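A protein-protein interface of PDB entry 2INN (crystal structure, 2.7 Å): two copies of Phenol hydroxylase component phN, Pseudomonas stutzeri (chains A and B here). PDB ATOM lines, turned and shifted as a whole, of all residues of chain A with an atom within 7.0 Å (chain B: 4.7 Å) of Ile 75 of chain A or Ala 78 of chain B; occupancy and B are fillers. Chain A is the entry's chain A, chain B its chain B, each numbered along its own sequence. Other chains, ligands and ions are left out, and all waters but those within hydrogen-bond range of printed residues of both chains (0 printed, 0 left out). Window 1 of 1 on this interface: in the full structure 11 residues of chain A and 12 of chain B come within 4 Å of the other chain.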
ATOM      1  N   GLU A  69       7.147  20.619  11.944  1.00  0.00           N
ATOM      2  CA  GLU A  69       5.660  20.656  11.898  1.00  0.00           C
ATOM      3  C   GLU A  69       5.158  22.025  12.245  1.00  0.00           C
ATOM      4  O   GLU A  69       4.319  22.512  11.560  1.00  0.00           O
ATOM      5  CB  GLU A  69       4.991  19.559  12.708  1.00  0.00           C
ATOM      6  CG  GLU A  69       5.184  18.239  12.090  1.00  0.00           C
ATOM      7  CD  GLU A  69       4.202  17.925  10.990  1.00  0.00           C
ATOM      8  OE1 GLU A  69       4.461  17.672   9.779  1.00  0.00           O
ATOM      9  OE2 GLU A  69       3.070  17.871  11.410  1.00  0.00           O
ATOM     10  N   LYS A  70       5.747  22.670  13.230  1.00  0.00           N
ATOM     11  CA  LYS A  70       5.266  23.971  13.687  1.00  0.00           C
ATOM     12  C   LYS A  70       5.368  24.956  12.582  1.00  0.00           C
ATOM     13  O   LYS A  70       4.453  25.710  12.361  1.00  0.00           O
ATOM     14  CB  LYS A  70       6.024  24.455  14.874  1.00  0.00           C
ATOM     15  CG  LYS A  70       5.078  24.838  15.956  1.00  0.00           C
ATOM     16  CD  LYS A  70       5.675  24.699  17.372  1.00  0.00           C
ATOM     17  CE  LYS A  70       6.052  23.262  17.709  1.00  0.00           C
ATOM     18  NZ  LYS A  70       6.716  23.284  19.004  1.00  0.00           N
ATOM     19  N   LYS A  71       6.413  24.870  11.783  1.00  0.00           N
ATOM     20  CA  LYS A  71       6.570  25.827  10.731  1.00  0.00           C
ATOM     21  C   LYS A  71       5.629  25.576   9.666  1.00  0.00           C
ATOM     22  O   LYS A  71       5.372  26.460   8.921  1.00  0.00           O
ATOM     23  CB  LYS A  71       7.954  25.782  10.126  1.00  0.00           C
ATOM     24  CG  LYS A  71       9.054  26.299  11.133  1.00  0.00           C
ATOM     25  CD  LYS A  71      10.410  26.217  10.450  1.00  0.00           C
ATOM     26  CE  LYS A  71      11.429  26.724  11.397  1.00  0.00           C
ATOM     27  NZ  LYS A  71      12.836  26.492  10.867  1.00  0.00           N
ATOM     28  N   LEU A  72       5.133  24.369   9.509  1.00  0.00           N
ATOM     29  CA  LEU A  72       4.380  24.086   8.291  1.00  0.00           C
ATOM     30  C   LEU A  72       2.871  24.420   8.559  1.00  0.00           C
ATOM     31  O   LEU A  72       2.113  24.792   7.634  1.00  0.00           O
ATOM     32  CB  LEU A  72       4.622  22.628   7.887  1.00  0.00           C
ATOM     33  CG  LEU A  72       3.697  21.879   6.940  1.00  0.00           C
ATOM     34  CD1 LEU A  72       4.193  22.058   5.531  1.00  0.00           C
ATOM     35  CD2 LEU A  72       3.700  20.458   7.286  1.00  0.00           C
ATOM     36  N   TYR A  73       2.444  24.314   9.826  1.00  0.00           N
ATOM     37  CA  TYR A  73       1.050  24.525  10.121  1.00  0.00           C
ATOM     38  C   TYR A  73       0.825  26.070  10.238  1.00  0.00           C
ATOM     39  O   TYR A  73      -0.148  26.570   9.739  1.00  0.00           O
ATOM     40  CB  TYR A  73       0.586  23.665  11.301  1.00  0.00           C
ATOM     41  CG  TYR A  73       0.239  22.229  10.907  1.00  0.00           C
ATOM     42  CD1 TYR A  73      -1.028  21.912  10.463  1.00  0.00           C
ATOM     43  CD2 TYR A  73       1.209  21.183  10.917  1.00  0.00           C
ATOM     44  CE1 TYR A  73      -1.362  20.626  10.083  1.00  0.00           C
ATOM     45  CE2 TYR A  73       0.875  19.907  10.495  1.00  0.00           C
ATOM     46  CZ  TYR A  73      -0.433  19.645  10.105  1.00  0.00           C
ATOM     47  OH  TYR A  73      -0.849  18.428   9.729  1.00  0.00           O
ATOM     48  N   ALA A  74       1.767  26.825  10.799  1.00  0.00           N
ATOM     49  CA  ALA A  74       1.711  28.241  10.602  1.00  0.00           C
ATOM     50  C   ALA A  74       1.449  28.641   9.147  1.00  0.00           C
ATOM     51  O   ALA A  74       0.513  29.463   8.883  1.00  0.00           O
ATOM     52  CB  ALA A  74       2.951  28.865  11.040  1.00  0.00           C
ATOM     53  N   ILE A  75       2.263  28.100   8.222  1.00  0.00           N
ATOM     54  CA  ILE A  75       2.076  28.418   6.801  1.00  0.00           C
ATOM     55  C   ILE A  75       0.734  27.855   6.309  1.00  0.00           C
ATOM     56  O   ILE A  75       0.050  28.595   5.562  1.00  0.00           O
ATOM     57  CB  ILE A  75       3.204  27.926   5.924  1.00  0.00           C
ATOM     58  CG1 ILE A  75       4.412  28.751   6.183  1.00  0.00           C
ATOM     59  CG2 ILE A  75       2.947  28.103   4.468  1.00  0.00           C
ATOM     60  CD1 ILE A  75       5.757  28.017   6.096  1.00  0.00           C
ATOM     61  N   PHE A  76       0.317  26.626   6.704  1.00  0.00           N
ATOM     62  CA  PHE A  76      -1.020  26.169   6.282  1.00  0.00           C
ATOM     63  C   PHE A  76      -2.139  27.135   6.787  1.00  0.00           C
ATOM     64  O   PHE A  76      -2.975  27.614   6.025  1.00  0.00           O
ATOM     65  CB  PHE A  76      -1.365  24.773   6.804  1.00  0.00           C
ATOM     66  CG  PHE A  76      -0.670  23.638   6.142  1.00  0.00           C
ATOM     67  CD1 PHE A  76      -0.026  23.764   4.875  1.00  0.00           C
ATOM     68  CD2 PHE A  76      -0.607  22.384   6.824  1.00  0.00           C
ATOM     69  CE1 PHE A  76       0.666  22.630   4.299  1.00  0.00           C
ATOM     70  CE2 PHE A  76       0.061  21.294   6.239  1.00  0.00           C
ATOM     71  CZ  PHE A  76       0.686  21.429   4.999  1.00  0.00           C
ATOM     72  N   ASP A  77      -2.169  27.351   8.102  1.00  0.00           N
ATOM     73  CA  ASP A  77      -2.980  28.382   8.718  1.00  0.00           C
ATOM     74  C   ASP A  77      -2.936  29.653   8.001  1.00  0.00           C
ATOM     75  O   ASP A  77      -3.991  30.072   7.633  1.00  0.00           O
ATOM     76  CB  ASP A  77      -2.680  28.658  10.172  1.00  0.00           C
ATOM     77  CG  ASP A  77      -2.819  27.381  11.022  1.00  0.00           C
ATOM     78  OD1 ASP A  77      -1.923  27.201  11.959  1.00  0.00           O
ATOM     79  OD2 ASP A  77      -3.713  26.531  10.649  1.00  0.00           O
ATOM     80  N   ALA A  78      -1.773  30.266   7.751  1.00  0.00           N
ATOM     81  CA  ALA A  78      -1.786  31.548   7.017  1.00  0.00           C
ATOM     82  C   ALA A  78      -2.445  31.316   5.666  1.00  0.00           C
ATOM     83  O   ALA A  78      -3.386  32.045   5.306  1.00  0.00           O
ATOM     84  CB  ALA A  78      -0.416  32.136   6.847  1.00  0.00           C
ATOM     85  N   PHE A  79      -2.056  30.260   4.953  1.00  0.00           N
ATOM     86  CA  PHE A  79      -2.473  30.118   3.570  1.00  0.00           C
ATOM     87  C   PHE A  79      -3.964  30.152   3.492  1.00  0.00           C
ATOM     88  O   PHE A  79      -4.540  30.831   2.654  1.00  0.00           O
ATOM     89  CB  PHE A  79      -2.027  28.782   3.081  1.00  0.00           C
ATOM     90  CG  PHE A  79      -2.491  28.454   1.737  1.00  0.00           C
ATOM     91  CD1 PHE A  79      -1.798  28.927   0.615  1.00  0.00           C
ATOM     92  CD2 PHE A  79      -3.581  27.590   1.576  1.00  0.00           C
ATOM     93  CE1 PHE A  79      -2.222  28.568  -0.722  1.00  0.00           C
ATOM     94  CE2 PHE A  79      -4.006  27.174   0.300  1.00  0.00           C
ATOM     95  CZ  PHE A  79      -3.318  27.698  -0.882  1.00  0.00           C
ATOM     96  N   ALA A  80      -4.573  29.424   4.399  1.00  0.00           N
ATOM     97  CA  ALA A  80      -5.989  29.363   4.463  1.00  0.00           C
ATOM     98  C   ALA A  80      -6.615  30.691   4.849  1.00  0.00           C
ATOM     99  O   ALA A  80      -7.663  30.974   4.390  1.00  0.00           O
ATOM    100  CB  ALA A  80      -6.408  28.303   5.443  1.00  0.00           C
ATOM    101  N   GLN A  81      -5.972  31.533   5.637  1.00  0.00           N
ATOM    102  CA  GLN A  81      -6.633  32.687   6.225  1.00  0.00           C
ATOM    103  C   GLN A  81      -6.593  33.861   5.192  1.00  0.00           C
ATOM    104  O   GLN A  81      -7.219  34.923   5.404  1.00  0.00           O
ATOM    105  CB  GLN A  81      -6.054  33.005   7.640  1.00  0.00           C
ATOM    106  CG  GLN A  81      -5.852  34.488   7.956  1.00  0.00           C
ATOM    107  CD  GLN A  81      -5.233  34.902   9.408  1.00  0.00           C
ATOM    108  OE1 GLN A  81      -4.891  34.061  10.275  1.00  0.00           O
ATOM    109  NE2 GLN A  81      -5.142  36.279   9.656  1.00  0.00           N
ATOM    110  N   MET A 220       1.194  27.736  -2.826  1.00  0.00           N
ATOM    111  CA  MET A 220       2.071  27.785  -1.721  1.00  0.00           C
ATOM    112  C   MET A 220       1.907  26.615  -0.749  1.00  0.00           C
ATOM    113  O   MET A 220       2.892  26.112  -0.221  1.00  0.00           O
ATOM    114  CB  MET A 220       1.954  29.102  -1.022  1.00  0.00           C
ATOM    115  CG  MET A 220       2.908  29.251   0.146  1.00  0.00           C
ATOM    116  SD  MET A 220       2.359  30.888   1.300  1.00  0.00           S
ATOM    117  CE  MET A 220       4.210  31.625   1.395  1.00  0.00           C
ATOM    118  N   ALA A 221       0.701  26.196  -0.453  1.00  0.00           N
ATOM    119  CA  ALA A 221       0.630  25.225   0.623  1.00  0.00           C
ATOM    120  C   ALA A 221       1.288  23.919   0.212  1.00  0.00           C
ATOM    121  O   ALA A 221       1.961  23.309   1.030  1.00  0.00           O
ATOM    122  CB  ALA A 221      -0.792  25.004   1.148  1.00  0.00           C
ATOM    123  N   THR A 224       5.240  24.069   0.306  1.00  0.00           N
ATOM    124  CA  THR A 224       5.716  23.969   1.682  1.00  0.00           C
ATOM    125  C   THR A 224       5.649  22.499   2.162  1.00  0.00           C
ATOM    126  O   THR A 224       6.518  22.011   2.890  1.00  0.00           O
ATOM    127  CB  THR A 224       4.809  24.817   2.482  1.00  0.00           C
ATOM    128  OG1 THR A 224       4.680  26.006   1.714  1.00  0.00           O
ATOM    129  CG2 THR A 224       5.289  25.159   3.913  1.00  0.00           C
ATOM    130  N   ALA B  74       8.148  31.816   9.986  1.00  0.00           N
ATOM    131  CA  ALA B  74       7.898  30.775   8.993  1.00  0.00           C
ATOM    132  C   ALA B  74       7.155  31.390   7.783  1.00  0.00           C
ATOM    133  O   ALA B  74       7.462  31.201   6.588  1.00  0.00           O
ATOM    134  CB  ALA B  74       7.114  29.722   9.613  1.00  0.00           C
ATOM    135  N   ILE B  75       6.204  32.230   8.125  1.00  0.00           N
ATOM    136  CA  ILE B  75       5.381  32.820   7.107  1.00  0.00           C
ATOM    137  C   ILE B  75       6.194  33.795   6.299  1.00  0.00           C
ATOM    138  O   ILE B  75       6.131  33.788   5.063  1.00  0.00           O
ATOM    139  CB  ILE B  75       4.194  33.553   7.771  1.00  0.00           C
ATOM    140  CG1 ILE B  75       3.437  32.574   8.663  1.00  0.00           C
ATOM    141  CG2 ILE B  75       3.376  34.317   6.748  1.00  0.00           C
ATOM    142  CD1 ILE B  75       2.073  33.002   8.967  1.00  0.00           C
ATOM    143  N   PHE B  76       6.959  34.641   6.981  1.00  0.00           N
ATOM    144  CA  PHE B  76       7.772  35.640   6.249  1.00  0.00           C
ATOM    145  C   PHE B  76       8.662  34.977   5.229  1.00  0.00           C
ATOM    146  O   PHE B  76       8.686  35.369   4.107  1.00  0.00           O
ATOM    147  CB  PHE B  76       8.689  36.302   7.213  1.00  0.00           C
ATOM    148  CG  PHE B  76       8.075  37.413   8.004  1.00  0.00           C
ATOM    149  CD1 PHE B  76       6.809  37.931   7.678  1.00  0.00           C
ATOM    150  CD2 PHE B  76       8.804  37.974   9.083  1.00  0.00           C
ATOM    151  CE1 PHE B  76       6.271  38.989   8.444  1.00  0.00           C
ATOM    152  CE2 PHE B  76       8.289  39.060   9.819  1.00  0.00           C
ATOM    153  CZ  PHE B  76       7.013  39.553   9.487  1.00  0.00           C
ATOM    154  N   ASP B  77       9.382  33.937   5.673  1.00  0.00           N
ATOM    155  CA  ASP B  77      10.230  33.081   4.869  1.00  0.00           C
ATOM    156  C   ASP B  77       9.488  32.508   3.701  1.00  0.00           C
ATOM    157  O   ASP B  77      10.054  32.583   2.575  1.00  0.00           O
ATOM    158  CB  ASP B  77      10.879  31.995   5.689  1.00  0.00           C
ATOM    159  CG  ASP B  77      12.048  32.531   6.610  1.00  0.00           C
ATOM    160  OD1 ASP B  77      12.309  33.781   6.724  1.00  0.00           O
ATOM    161  OD2 ASP B  77      12.716  31.729   7.314  1.00  0.00           O
ATOM    162  N   ALA B  78       8.271  31.969   3.925  1.00  0.00           N
ATOM    163  CA  ALA B  78       7.492  31.364   2.840  1.00  0.00           C
ATOM    164  C   ALA B  78       7.011  32.434   1.803  1.00  0.00           C
ATOM    165  O   ALA B  78       7.343  32.343   0.592  1.00  0.00           O
ATOM    166  CB  ALA B  78       6.312  30.689   3.381  1.00  0.00           C
ATOM    167  N   PHE B  79       6.236  33.447   2.242  1.00  0.00           N
ATOM    168  CA  PHE B  79       6.111  34.611   1.461  1.00  0.00           C
ATOM    169  C   PHE B  79       7.335  34.929   0.517  1.00  0.00           C
ATOM    170  O   PHE B  79       7.159  35.163  -0.672  1.00  0.00           O
ATOM    171  CB  PHE B  79       5.840  35.781   2.372  1.00  0.00           C
ATOM    172  CG  PHE B  79       5.304  36.940   1.635  1.00  0.00           C
ATOM    173  CD1 PHE B  79       3.958  36.976   1.270  1.00  0.00           C
ATOM    174  CD2 PHE B  79       6.154  37.950   1.200  1.00  0.00           C
ATOM    175  CE1 PHE B  79       3.463  38.032   0.563  1.00  0.00           C
ATOM    176  CE2 PHE B  79       5.677  39.014   0.487  1.00  0.00           C
ATOM    177  CZ  PHE B  79       4.311  39.021   0.183  1.00  0.00           C
ATOM    178  N   ALA B  80       8.557  34.964   1.062  1.00  0.00           N
ATOM    179  CA  ALA B  80       9.742  35.341   0.274  1.00  0.00           C
ATOM    180  C   ALA B  80      10.037  34.230  -0.730  1.00  0.00           C
ATOM    181  O   ALA B  80       9.822  34.448  -1.924  1.00  0.00           O
ATOM    182  CB  ALA B  80      10.996  35.656   1.180  1.00  0.00           C
ATOM    183  N   GLN B  81      10.464  33.055  -0.219  1.00  0.00           N
ATOM    184  CA  GLN B  81      10.573  31.854  -0.989  1.00  0.00           C
ATOM    185  C   GLN B  81       9.636  31.832  -2.154  1.00  0.00           C
ATOM    186  O   GLN B  81      10.032  31.442  -3.204  1.00  0.00           O
ATOM    187  CB  GLN B  81      10.321  30.577  -0.120  1.00  0.00           C
ATOM    188  CG  GLN B  81      11.519  29.465  -0.172  1.00  0.00           C
ATOM    189  CD  GLN B  81      11.479  28.732  -1.512  1.00  0.00           C
ATOM    190  OE1 GLN B  81      10.385  28.504  -2.032  1.00  0.00           O
ATOM    191  NE2 GLN B  81      12.645  28.407  -2.108  1.00  0.00           N
ATOM    192  N   ASN B  82       8.413  32.271  -1.989  1.00  0.00           N
ATOM    193  CA  ASN B  82       7.424  32.013  -2.976  1.00  0.00           C
ATOM    194  C   ASN B  82       6.989  33.228  -3.801  1.00  0.00           C
ATOM    195  O   ASN B  82       6.004  33.170  -4.553  1.00  0.00           O
ATOM    196  CB  ASN B  82       6.191  31.491  -2.244  1.00  0.00           C
ATOM    197  CG  ASN B  82       6.232  29.956  -2.021  1.00  0.00           C
ATOM    198  OD1 ASN B  82       6.417  29.164  -2.985  1.00  0.00           O
ATOM    199  ND2 ASN B  82       6.023  29.536  -0.767  1.00  0.00           N
ATOM    200  N   ASN B  83       7.692  34.350  -3.603  1.00  0.00           N
ATOM    201  CA  ASN B  83       7.437  35.561  -4.348  1.00  0.00           C
ATOM    202  C   ASN B  83       6.029  36.007  -4.200  1.00  0.00           C
ATOM    203  O   ASN B  83       5.371  36.386  -5.146  1.00  0.00           O
ATOM    204  CB  ASN B  83       7.934  35.368  -5.779  1.00  0.00           C
ATOM    205  CG  ASN B  83       9.486  35.230  -5.809  1.00  0.00           C
ATOM    206  OD1 ASN B  83      10.177  35.897  -5.036  1.00  0.00           O
ATOM    207  ND2 ASN B  83      10.021  34.361  -6.666  1.00  0.00           N
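ND2 of Asn 82 of chain B lies close to O of Ala 78 of chain B (3.4 Å). The side-chain hydroxyl (OG1) of Thr 224 of chain A sits at hydrogen-bond distance from the backbone carbonyl oxygen (O) of Met 220 of chain A (2.6 Å).
Lys 71 of chain A touches Ala 74 of chain B. Ala 74 of chain A touches Ile 75 of chain B (O to CD1, 3.9 Å). Ile 75 of chain A touches Ala 74 of chain B (CD1 to O, 3.6 Å). Ala 78 of chain B touches Ile 75 of chain A. CB of Ala 78 of chain A touches CD1 of Ile 75 of chain B, at 3.4 Å. Met 220 of chain A touches Ala 78 of chain B. Met 220 of chain A touches Phe 79 of chain B. Asn 82 of chain B touches Met 220 of chain A (ND2 to CG, 3.3 Å).
Ile 75 of chain A touches two residues of chain B. Ala 78 of chain B touches just these residues of chain A: Ile 75 and Met 220. Printed residues of chain B within 4 Å of Ala 74 of chain A: Ile 75 (3.9 Å). Of the printed residues of chain A, Asn 82 of chain B touches Met 220 (3.3 Å). Phe 79 of chain A touches none of the printed residues of chain B.
Of the 16 printed residues of chain A, 5 touch a printed residue of chain B. Hydrophobic or aromatic side chains of chain A within 4 Å of the printed part of chain B: Ile 75, Ala 78 and Met 220. Of the 10 printed residues of chain B, 5 touch a printed residue of chain A.
Ala 74 of chain A touches Ile 75 of chain B, and with the chains exchanged Ile 75 of chain A touches Ala 74 of chain B. Ile 75 of chain A touches Ala 78 of chain B, and with the chains exchanged Ala 78 of chain A touches Ile 75 of chain B.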
